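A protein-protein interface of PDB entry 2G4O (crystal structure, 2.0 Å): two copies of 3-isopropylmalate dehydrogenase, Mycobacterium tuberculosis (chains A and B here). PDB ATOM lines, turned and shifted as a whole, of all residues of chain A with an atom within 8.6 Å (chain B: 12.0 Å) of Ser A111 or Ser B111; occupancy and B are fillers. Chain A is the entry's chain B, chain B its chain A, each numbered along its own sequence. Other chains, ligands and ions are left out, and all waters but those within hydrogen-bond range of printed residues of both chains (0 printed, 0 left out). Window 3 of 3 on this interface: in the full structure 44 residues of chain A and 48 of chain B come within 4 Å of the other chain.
N of Ser A111 lies within hydrogen-bond range of O of Pro B109, at 2.8 Å. The backbone NH (N) of Ser B111 is in hydrogen-bond range of the backbone carbonyl oxygen (O) of Pro A109 (2.9 Å).
The side-chain hydroxyl (OG) of Ser B108 lies close to the backbone NH (N) of Leu B110, 3.1 Å away. The side-chain hydroxyl of Ser B108 lies within hydrogen-bond range of the backbone carbonyl oxygen of Val B245 (2.9 Å). OG of Ser A108 is in hydrogen-bond range of N of Leu A110 (3.0 Å).
Leu B110 touches Pro A109. CG2 of Ile B219 touches CG of Pro A109, at 3.7 Å. Pro B109 touches Leu A110 (O to CA, 3.7 Å). Leu A110 touches Ser B111 (C to N, 3.8 Å). Leu B110 touches Ser A111. Ser A111 touches Ser B111 (N to N, 3.6 Å). Pro B109 touches Ile A219. Ile A219 touches Ile B219 (CG2 to CD1, 3.9 Å). Ala B244 touches Ile A219. CD1 of Ile A219 touches CG1 of Val B245, at 3.5 Å.
No residue of chain B comes within 4 Å of Ser A108. Printed residues of chain B within 4 Å of Pro A109: Leu B110 (3.7 Å), Ser B111 (2.9 Å) and Ile B219 (3.7 Å). Leu A110 touches just these residues of chain B: Pro B109 and Ser B111. No residue of chain B comes within 4 Å of Gly A112. Asn A113 touches none of the printed residues of chain B. No residue of chain B comes within 4 Å of Pro A114. Printed residues of chain B within 4 Å of Ile A219: Pro B109 (3.6 Å), Ile B219 (3.9 Å), Ala B244 (3.5 Å) and Val B245 (3.5 Å). Printed residues of chain A within 4 Å of Leu B110: Pro A109 (3.7 Å) and Ser A111 (3.8 Å). Ser B111 touches just these residues of chain A: Pro A109, Leu A110 and Ser A111. No residue of chain A comes within 4 Å of Gly B112. Ile B216 touches none of the printed residues of chain A. Of the printed residues of chain A, Val B245 touches Ile A219.
Hydrophobic or aromatic side chains of chain B within 4 Å of the printed part of chain A: Pro B109, Leu B110, Ile B219, Ala B244 and Val B245. Of the 15 printed residues of chain A, 4 touch a printed residue of chain B. Hydrophobic or aromatic side chains of chain A that line the printed part of chain B: Pro A109, Leu A110 and Ile A219. Among the printed residues, 12 pairs touch across the chains.
Pro A109 touches Leu B110, and with the chains exchanged Leu A110 touches Pro B109. Pro A109 touches Ile B219, and with the chains exchanged Ile A219 touches Pro B109. Ile B219 touches its own counterpart, Ile A219. Ile A219 touches Val B245, but with the chains exchanged Val A245 does not touch Ile B219 (4.3 Å). Positions printed for both chains: 102, 107, 108, 109, 110, 111, 112, 113, 114, 115, 116, 219, 220, 222 and 245. Of the 12 pairs that touch across the chains among the printed residues, 10 have their exchanged pair printed and touching as well.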
ATOM      1  N   LEU A 102      22.632 -14.259  19.002  1.00  0.00           N
ATOM      2  CA  LEU A 102      23.637 -15.003  18.275  1.00  0.00           C
ATOM      3  C   LEU A 102      24.536 -15.633  19.361  1.00  0.00           C
ATOM      4  O   LEU A 102      25.149 -14.915  20.142  1.00  0.00           O
ATOM      5  CB  LEU A 102      24.466 -14.091  17.366  1.00  0.00           C
ATOM      6  CG  LEU A 102      25.484 -14.766  16.434  1.00  0.00           C
ATOM      7  CD1 LEU A 102      24.904 -15.991  15.661  1.00  0.00           C
ATOM      8  CD2 LEU A 102      26.089 -13.791  15.462  1.00  0.00           C
ATOM      9  N   ALA A 107      27.000 -19.450  13.440  1.00  0.00           N
ATOM     10  CA  ALA A 107      27.472 -18.506  12.426  1.00  0.00           C
ATOM     11  C   ALA A 107      26.316 -17.622  11.933  1.00  0.00           C
ATOM     12  O   ALA A 107      25.257 -18.104  11.500  1.00  0.00           O
ATOM     13  CB  ALA A 107      28.112 -19.233  11.258  1.00  0.00           C
ATOM     14  N   SER A 108      26.557 -16.324  12.004  1.00  0.00           N
ATOM     15  CA  SER A 108      25.681 -15.326  11.408  1.00  0.00           C
ATOM     16  C   SER A 108      26.041 -15.029   9.930  1.00  0.00           C
ATOM     17  O   SER A 108      27.230 -14.911   9.587  1.00  0.00           O
ATOM     18  CB  SER A 108      25.779 -14.048  12.214  1.00  0.00           C
ATOM     19  OG  SER A 108      25.355 -12.956  11.460  1.00  0.00           O
ATOM     20  N   PRO A 109      25.003 -14.819   9.090  1.00  0.00           N
ATOM     21  CA  PRO A 109      25.203 -14.512   7.677  1.00  0.00           C
ATOM     22  C   PRO A 109      25.717 -13.079   7.495  1.00  0.00           C
ATOM     23  O   PRO A 109      26.003 -12.653   6.361  1.00  0.00           O
ATOM     24  CB  PRO A 109      23.807 -14.696   7.082  1.00  0.00           C
ATOM     25  CG  PRO A 109      22.894 -14.308   8.213  1.00  0.00           C
ATOM     26  CD  PRO A 109      23.573 -14.795   9.461  1.00  0.00           C
ATOM     27  N   LEU A 110      25.823 -12.362   8.608  1.00  0.00           N
ATOM     28  CA  LEU A 110      26.358 -11.029   8.633  1.00  0.00           C
ATOM     29  C   LEU A 110      27.843 -11.071   8.841  1.00  0.00           C
ATOM     30  O   LEU A 110      28.359 -12.006   9.458  1.00  0.00           O
ATOM     31  CB  LEU A 110      25.789 -10.237   9.815  1.00  0.00           C
ATOM     32  CG  LEU A 110      24.329  -9.749   9.805  1.00  0.00           C
ATOM     33  CD1 LEU A 110      24.199  -8.844  10.974  1.00  0.00           C
ATOM     34  CD2 LEU A 110      23.976  -8.955   8.540  1.00  0.00           C
ATOM     35  N   SER A 111      28.494  -9.994   8.401  1.00  0.00           N
ATOM     36  CA  SER A 111      29.932  -9.796   8.550  1.00  0.00           C
ATOM     37  C   SER A 111      30.412  -9.718  10.026  1.00  0.00           C
ATOM     38  O   SER A 111      29.861  -8.955  10.834  1.00  0.00           O
ATOM     39  CB  SER A 111      30.339  -8.516   7.812  1.00  0.00           C
ATOM     40  OG  SER A 111      31.719  -8.333   7.908  1.00  0.00           O
ATOM     41  N   GLY A 112      31.448 -10.521  10.339  1.00  0.00           N
ATOM     42  CA  GLY A 112      32.231 -10.408  11.579  1.00  0.00           C
ATOM     43  C   GLY A 112      31.571 -10.849  12.875  1.00  0.00           C
ATOM     44  O   GLY A 112      31.803 -10.228  13.930  1.00  0.00           O
ATOM     45  N   ASN A 113      30.764 -11.912  12.843  1.00  0.00           N
ATOM     46  CA  ASN A 113      30.128 -12.441  14.098  1.00  0.00           C
ATOM     47  C   ASN A 113      29.946 -11.362  15.214  1.00  0.00           C
ATOM     48  O   ASN A 113      30.559 -11.478  16.291  1.00  0.00           O
ATOM     49  CB  ASN A 113      30.950 -13.632  14.661  1.00  0.00           C
ATOM     50  CG  ASN A 113      30.160 -14.488  15.667  1.00  0.00           C
ATOM     51  OD1 ASN A 113      29.819 -15.633  15.376  1.00  0.00           O
ATOM     52  ND2 ASN A 113      29.845 -13.925  16.830  1.00  0.00           N
ATOM     53  N   PRO A 114      29.085 -10.332  14.974  1.00  0.00           N
ATOM     54  CA  PRO A 114      28.935  -9.171  15.862  1.00  0.00           C
ATOM     55  C   PRO A 114      28.171  -9.502  17.142  1.00  0.00           C
ATOM     56  O   PRO A 114      27.629 -10.585  17.264  1.00  0.00           O
ATOM     57  CB  PRO A 114      28.102  -8.195  15.016  1.00  0.00           C
ATOM     58  CG  PRO A 114      27.253  -9.088  14.201  1.00  0.00           C
ATOM     59  CD  PRO A 114      28.143 -10.258  13.836  1.00  0.00           C
ATOM     60  N   GLY A 115      28.121  -8.578  18.089  1.00  0.00           N
ATOM     61  CA  GLY A 115      27.344  -8.824  19.307  1.00  0.00           C
ATOM     62  C   GLY A 115      25.866  -8.629  18.980  1.00  0.00           C
ATOM     63  O   GLY A 115      25.486  -7.550  18.513  1.00  0.00           O
ATOM     64  N   ILE A 116      25.060  -9.675  19.153  1.00  0.00           N
ATOM     65  CA  ILE A 116      23.597  -9.582  18.946  1.00  0.00           C
ATOM     66  C   ILE A 116      22.867 -10.347  20.051  1.00  0.00           C
ATOM     67  O   ILE A 116      22.951 -11.601  20.148  1.00  0.00           O
ATOM     68  CB  ILE A 116      23.094 -10.206  17.608  1.00  0.00           C
ATOM     69  CG1 ILE A 116      23.856  -9.685  16.392  1.00  0.00           C
ATOM     70  CG2 ILE A 116      21.560  -9.934  17.432  1.00  0.00           C
ATOM     71  CD1 ILE A 116      23.605 -10.491  15.160  1.00  0.00           C
ATOM     72  N   ILE A 219      20.819  -5.237  10.199  1.00  0.00           N
ATOM     73  CA  ILE A 219      21.900  -5.845   9.490  1.00  0.00           C
ATOM     74  C   ILE A 219      23.232  -5.094   9.554  1.00  0.00           C
ATOM     75  O   ILE A 219      24.289  -5.730   9.417  1.00  0.00           O
ATOM     76  CB  ILE A 219      21.535  -6.164   8.041  1.00  0.00           C
ATOM     77  CG1 ILE A 219      21.685  -4.955   7.138  1.00  0.00           C
ATOM     78  CG2 ILE A 219      20.139  -6.755   7.956  1.00  0.00           C
ATOM     79  CD1 ILE A 219      21.768  -5.359   5.698  1.00  0.00           C
ATOM     80  N   THR A 220      23.204  -3.775   9.729  1.00  0.00           N
ATOM     81  CA  THR A 220      24.439  -3.037   9.835  1.00  0.00           C
ATOM     82  C   THR A 220      24.855  -2.759  11.288  1.00  0.00           C
ATOM     83  O   THR A 220      26.028  -2.554  11.543  1.00  0.00           O
ATOM     84  CB  THR A 220      24.397  -1.684   9.116  1.00  0.00           C
ATOM     85  OG1 THR A 220      23.622  -0.752   9.879  1.00  0.00           O
ATOM     86  CG2 THR A 220      23.866  -1.821   7.705  1.00  0.00           C
ATOM     87  N   PRO A 222      23.166  -4.302  14.567  1.00  0.00           N
ATOM     88  CA  PRO A 222      22.150  -4.959  15.388  1.00  0.00           C
ATOM     89  C   PRO A 222      22.422  -4.859  16.865  1.00  0.00           C
ATOM     90  O   PRO A 222      21.544  -5.179  17.681  1.00  0.00           O
ATOM     91  CB  PRO A 222      22.195  -6.417  14.947  1.00  0.00           C
ATOM     92  CG  PRO A 222      23.443  -6.556  14.106  1.00  0.00           C
ATOM     93  CD  PRO A 222      23.930  -5.236  13.720  1.00  0.00           C
ATOM     94  N   VAL A 245      19.675 -13.323  11.059  1.00  0.00           N
ATOM     95  CA  VAL A 245      20.965 -12.747  11.422  1.00  0.00           C
ATOM     96  C   VAL A 245      21.579 -13.417  12.656  1.00  0.00           C
ATOM     97  O   VAL A 245      22.771 -13.278  12.891  1.00  0.00           O
ATOM     98  CB  VAL A 245      20.932 -11.219  11.726  1.00  0.00           C
ATOM     99  CG1 VAL A 245      20.508 -10.410  10.531  1.00  0.00           C
ATOM    100  CG2 VAL A 245      20.095 -10.869  12.964  1.00  0.00           C
ATOM    101  N   LEU B 102      25.782  -4.865  -6.027  1.00  0.00           N
ATOM    102  CA  LEU B 102      26.983  -4.733  -5.201  1.00  0.00           C
ATOM    103  C   LEU B 102      28.209  -4.653  -6.104  1.00  0.00           C
ATOM    104  O   LEU B 102      28.482  -5.575  -6.885  1.00  0.00           O
ATOM    105  CB  LEU B 102      27.087  -5.884  -4.186  1.00  0.00           C
ATOM    106  CG  LEU B 102      28.283  -5.796  -3.232  1.00  0.00           C
ATOM    107  CD1 LEU B 102      28.303  -4.497  -2.348  1.00  0.00           C
ATOM    108  CD2 LEU B 102      28.346  -7.046  -2.423  1.00  0.00           C
ATOM    109  N   VAL B 106      32.903  -1.571  -2.949  1.00  0.00           N
ATOM    110  CA  VAL B 106      31.844  -1.301  -1.941  1.00  0.00           C
ATOM    111  C   VAL B 106      31.754  -2.485  -1.021  1.00  0.00           C
ATOM    112  O   VAL B 106      31.631  -3.625  -1.473  1.00  0.00           O
ATOM    113  CB  VAL B 106      30.437  -1.025  -2.612  1.00  0.00           C
ATOM    114  CG1 VAL B 106      29.346  -0.741  -1.563  1.00  0.00           C
ATOM    115  CG2 VAL B 106      30.525   0.174  -3.542  1.00  0.00           C
ATOM    116  N   ALA B 107      31.834  -2.207   0.279  1.00  0.00           N
ATOM    117  CA  ALA B 107      31.594  -3.188   1.322  1.00  0.00           C
ATOM    118  C   ALA B 107      30.124  -3.461   1.633  1.00  0.00           C
ATOM    119  O   ALA B 107      29.339  -2.547   1.900  1.00  0.00           O
ATOM    120  CB  ALA B 107      32.319  -2.760   2.602  1.00  0.00           C
ATOM    121  N   SER B 108      29.764  -4.745   1.607  1.00  0.00           N
ATOM    122  CA  SER B 108      28.512  -5.245   2.085  1.00  0.00           C
ATOM    123  C   SER B 108      28.601  -5.585   3.574  1.00  0.00           C
ATOM    124  O   SER B 108      29.647  -6.026   4.058  1.00  0.00           O
ATOM    125  CB  SER B 108      28.187  -6.476   1.274  1.00  0.00           C
ATOM    126  OG  SER B 108      26.983  -7.084   1.667  1.00  0.00           O
ATOM    127  N   PRO B 109      27.506  -5.415   4.323  1.00  0.00           N
ATOM    128  CA  PRO B 109      27.453  -5.913   5.698  1.00  0.00           C
ATOM    129  C   PRO B 109      27.234  -7.414   5.777  1.00  0.00           C
ATOM    130  O   PRO B 109      27.267  -7.966   6.855  1.00  0.00           O
ATOM    131  CB  PRO B 109      26.234  -5.182   6.266  1.00  0.00           C
ATOM    132  CG  PRO B 109      25.347  -5.036   5.083  1.00  0.00           C
ATOM    133  CD  PRO B 109      26.263  -4.730   3.958  1.00  0.00           C
ATOM    134  N   LEU B 110      27.032  -8.083   4.653  1.00  0.00           N
ATOM    135  CA  LEU B 110      26.942  -9.540   4.668  1.00  0.00           C
ATOM    136  C   LEU B 110      28.314 -10.208   4.606  1.00  0.00           C
ATOM    137  O   LEU B 110      29.261  -9.665   4.054  1.00  0.00           O
ATOM    138  CB  LEU B 110      26.086 -10.065   3.517  1.00  0.00           C
ATOM    139  CG  LEU B 110      24.704  -9.407   3.277  1.00  0.00           C
ATOM    140  CD1 LEU B 110      24.061 -10.146   2.150  1.00  0.00           C
ATOM    141  CD2 LEU B 110      23.826  -9.464   4.542  1.00  0.00           C
ATOM    142  N   SER B 111      28.385 -11.425   5.139  1.00  0.00           N
ATOM    143  CA  SER B 111      29.596 -12.240   5.071  1.00  0.00           C
ATOM    144  C   SER B 111      29.958 -12.631   3.603  1.00  0.00           C
ATOM    145  O   SER B 111      29.097 -12.920   2.791  1.00  0.00           O
ATOM    146  CB  SER B 111      29.404 -13.468   5.957  1.00  0.00           C
ATOM    147  OG  SER B 111      30.604 -14.202   6.090  1.00  0.00           O
ATOM    148  N   GLY B 112      31.235 -12.555   3.246  1.00  0.00           N
ATOM    149  CA  GLY B 112      31.736 -13.240   2.045  1.00  0.00           C
ATOM    150  C   GLY B 112      31.502 -12.692   0.635  1.00  0.00           C
ATOM    151  O   GLY B 112      31.445 -13.504  -0.334  1.00  0.00           O
ATOM    152  N   ASN B 113      31.417 -11.357   0.520  1.00  0.00           N
ATOM    153  CA  ASN B 113      31.213 -10.633  -0.747  1.00  0.00           C
ATOM    154  C   ASN B 113      30.349 -11.341  -1.805  1.00  0.00           C
ATOM    155  O   ASN B 113      30.819 -11.673  -2.888  1.00  0.00           O
ATOM    156  CB  ASN B 113      32.579 -10.252  -1.332  1.00  0.00           C
ATOM    157  CG  ASN B 113      32.488  -9.335  -2.551  1.00  0.00           C
ATOM    158  OD1 ASN B 113      31.538  -8.562  -2.678  1.00  0.00           O
ATOM    159  ND2 ASN B 113      33.509  -9.392  -3.446  1.00  0.00           N
ATOM    160  N   PRO B 114      29.056 -11.543  -1.508  1.00  0.00           N
ATOM    161  CA  PRO B 114      28.227 -12.294  -2.446  1.00  0.00           C
ATOM    162  C   PRO B 114      27.968 -11.472  -3.691  1.00  0.00           C
ATOM    163  O   PRO B 114      27.924 -10.236  -3.636  1.00  0.00           O
ATOM    164  CB  PRO B 114      26.917 -12.496  -1.662  1.00  0.00           C
ATOM    165  CG  PRO B 114      26.831 -11.261  -0.832  1.00  0.00           C
ATOM    166  CD  PRO B 114      28.259 -11.058  -0.363  1.00  0.00           C
ATOM    167  N   GLY B 115      27.777 -12.136  -4.823  1.00  0.00           N
ATOM    168  CA  GLY B 115      27.340 -11.391  -6.021  1.00  0.00           C
ATOM    169  C   GLY B 115      25.890 -10.964  -5.781  1.00  0.00           C
ATOM    170  O   GLY B 115      25.079 -11.779  -5.416  1.00  0.00           O
ATOM    171  N   ILE B 116      25.606  -9.670  -5.936  1.00  0.00           N
ATOM    172  CA  ILE B 116      24.258  -9.105  -5.790  1.00  0.00           C
ATOM    173  C   ILE B 116      24.016  -8.165  -6.998  1.00  0.00           C
ATOM    174  O   ILE B 116      24.785  -7.212  -7.275  1.00  0.00           O
ATOM    175  CB  ILE B 116      24.057  -8.325  -4.469  1.00  0.00           C
ATOM    176  CG1 ILE B 116      24.537  -9.147  -3.299  1.00  0.00           C
ATOM    177  CG2 ILE B 116      22.564  -7.941  -4.303  1.00  0.00           C
ATOM    178  CD1 ILE B 116      24.407  -8.514  -1.903  1.00  0.00           C
ATOM    179  N   ILE B 216      14.618 -12.574   4.762  1.00  0.00           N
ATOM    180  CA  ILE B 216      15.636 -13.549   5.082  1.00  0.00           C
ATOM    181  C   ILE B 216      16.546 -13.859   3.901  1.00  0.00           C
ATOM    182  O   ILE B 216      17.774 -13.828   4.024  1.00  0.00           O
ATOM    183  CB  ILE B 216      15.015 -14.864   5.586  1.00  0.00           C
ATOM    184  CG1 ILE B 216      14.229 -14.599   6.883  1.00  0.00           C
ATOM    185  CG2 ILE B 216      16.140 -15.963   5.771  1.00  0.00           C
ATOM    186  CD1 ILE B 216      13.620 -15.839   7.525  1.00  0.00           C
ATOM    187  N   HIS B 217      15.970 -14.167   2.750  1.00  0.00           N
ATOM    188  CA  HIS B 217      16.815 -14.413   1.558  1.00  0.00           C
ATOM    189  C   HIS B 217      17.688 -13.267   1.139  1.00  0.00           C
ATOM    190  O   HIS B 217      18.828 -13.496   0.726  1.00  0.00           O
ATOM    191  CB  HIS B 217      16.008 -14.924   0.376  1.00  0.00           C
ATOM    192  CG  HIS B 217      15.631 -16.361   0.522  1.00  0.00           C
ATOM    193  ND1 HIS B 217      14.335 -16.805   0.422  1.00  0.00           N
ATOM    194  CD2 HIS B 217      16.384 -17.449   0.812  1.00  0.00           C
ATOM    195  CE1 HIS B 217      14.304 -18.112   0.616  1.00  0.00           C
ATOM    196  NE2 HIS B 217      15.535 -18.527   0.867  1.00  0.00           N
ATOM    197  N   MET B 218      17.212 -12.030   1.262  1.00  0.00           N
ATOM    198  CA  MET B 218      18.066 -10.861   0.912  1.00  0.00           C
ATOM    199  C   MET B 218      19.395 -10.825   1.743  1.00  0.00           C
ATOM    200  O   MET B 218      20.397 -10.185   1.348  1.00  0.00           O
ATOM    201  CB  MET B 218      17.252  -9.563   1.079  1.00  0.00           C
ATOM    202  CG  MET B 218      17.578  -8.448   0.137  1.00  0.00           C
ATOM    203  SD  MET B 218      16.218  -7.231   0.014  1.00  0.00           S
ATOM    204  CE  MET B 218      14.995  -8.012  -1.029  1.00  0.00           C
ATOM    205  N   ILE B 219      19.367 -11.517   2.882  1.00  0.00           N
ATOM    206  CA  ILE B 219      20.468 -11.607   3.857  1.00  0.00           C
ATOM    207  C   ILE B 219      21.307 -12.881   3.655  1.00  0.00           C
ATOM    208  O   ILE B 219      22.502 -12.858   3.910  1.00  0.00           O
ATOM    209  CB  ILE B 219      19.853 -11.553   5.373  1.00  0.00           C
ATOM    210  CG1 ILE B 219      19.241 -10.163   5.632  1.00  0.00           C
ATOM    211  CG2 ILE B 219      20.845 -11.849   6.453  1.00  0.00           C
ATOM    212  CD1 ILE B 219      19.840  -9.037   4.811  1.00  0.00           C
ATOM    213  N   THR B 220      20.676 -13.977   3.258  1.00  0.00           N
ATOM    214  CA  THR B 220      21.360 -15.246   3.176  1.00  0.00           C
ATOM    215  C   THR B 220      21.625 -15.684   1.723  1.00  0.00           C
ATOM    216  O   THR B 220      22.563 -16.421   1.464  1.00  0.00           O
ATOM    217  CB  THR B 220      20.608 -16.335   3.946  1.00  0.00           C
ATOM    218  OG1 THR B 220      19.358 -16.597   3.318  1.00  0.00           O
ATOM    219  CG2 THR B 220      20.372 -15.936   5.424  1.00  0.00           C
ATOM    220  N   ASP B 221      20.849 -15.173   0.776  1.00  0.00           N
ATOM    221  CA  ASP B 221      20.906 -15.658  -0.584  1.00  0.00           C
ATOM    222  C   ASP B 221      20.539 -14.567  -1.600  1.00  0.00           C
ATOM    223  O   ASP B 221      19.758 -14.803  -2.547  1.00  0.00           O
ATOM    224  CB  ASP B 221      19.923 -16.822  -0.618  1.00  0.00           C
ATOM    225  CG  ASP B 221      20.031 -17.650  -1.842  1.00  0.00           C
ATOM    226  OD1 ASP B 221      21.040 -17.535  -2.587  1.00  0.00           O
ATOM    227  OD2 ASP B 221      19.066 -18.429  -2.020  1.00  0.00           O
ATOM    228  N   PRO B 222      21.104 -13.354  -1.427  1.00  0.00           N
ATOM    229  CA  PRO B 222      20.637 -12.257  -2.290  1.00  0.00           C
ATOM    230  C   PRO B 222      20.895 -12.460  -3.784  1.00  0.00           C
ATOM    231  O   PRO B 222      20.296 -11.787  -4.615  1.00  0.00           O
ATOM    232  CB  PRO B 222      21.386 -11.023  -1.749  1.00  0.00           C
ATOM    233  CG  PRO B 222      22.641 -11.591  -1.053  1.00  0.00           C
ATOM    234  CD  PRO B 222      22.101 -12.904  -0.435  1.00  0.00           C
ATOM    235  N   GLY B 223      21.793 -13.384  -4.120  1.00  0.00           N
ATOM    236  CA  GLY B 223      22.050 -13.735  -5.533  1.00  0.00           C
ATOM    237  C   GLY B 223      20.876 -14.411  -6.257  1.00  0.00           C
ATOM    238  O   GLY B 223      20.903 -14.494  -7.468  1.00  0.00           O
ATOM    239  N   ALA B 244      20.916  -1.421   1.930  1.00  0.00           N
ATOM    240  CA  ALA B 244      21.787  -1.869   3.018  1.00  0.00           C
ATOM    241  C   ALA B 244      22.723  -3.062   2.633  1.00  0.00           C
ATOM    242  O   ALA B 244      23.992  -3.030   2.915  1.00  0.00           O
ATOM    243  CB  ALA B 244      20.948  -2.220   4.258  1.00  0.00           C
ATOM    244  N   VAL B 245      22.165  -4.099   2.007  1.00  0.00           N
ATOM    245  CA  VAL B 245      23.070  -5.176   1.597  1.00  0.00           C
ATOM    246  C   VAL B 245      24.053  -4.779   0.453  1.00  0.00           C
ATOM    247  O   VAL B 245      25.075  -5.381   0.302  1.00  0.00           O
ATOM    248  CB  VAL B 245      22.347  -6.529   1.341  1.00  0.00           C
ATOM    249  CG1 VAL B 245      21.434  -6.921   2.597  1.00  0.00           C
ATOM    250  CG2 VAL B 245      21.566  -6.516   0.049  1.00  0.00           C
ATOM    251  N   CYS B 246      23.729  -3.766  -0.338  1.00  0.00           N
ATOM    252  CA  CYS B 246      24.563  -3.353  -1.438  1.00  0.00           C
ATOM    253  C   CYS B 246      25.490  -2.156  -1.018  1.00  0.00           C
ATOM    254  O   CYS B 246      26.054  -1.448  -1.853  1.00  0.00           O
ATOM    255  CB  CYS B 246      23.672  -3.025  -2.619  1.00  0.00           C
ATOM    256  SG  CYS B 246      23.019  -4.499  -3.376  1.00  0.00           S
ATOM    257  N   GLY B 247      25.639  -1.945   0.292  1.00  0.00           N
ATOM    258  CA  GLY B 247      26.617  -1.028   0.804  1.00  0.00           C
ATOM    259  C   GLY B 247      26.076   0.314   1.255  1.00  0.00           C
ATOM    260  O   GLY B 247      26.858   1.220   1.530  1.00  0.00           O
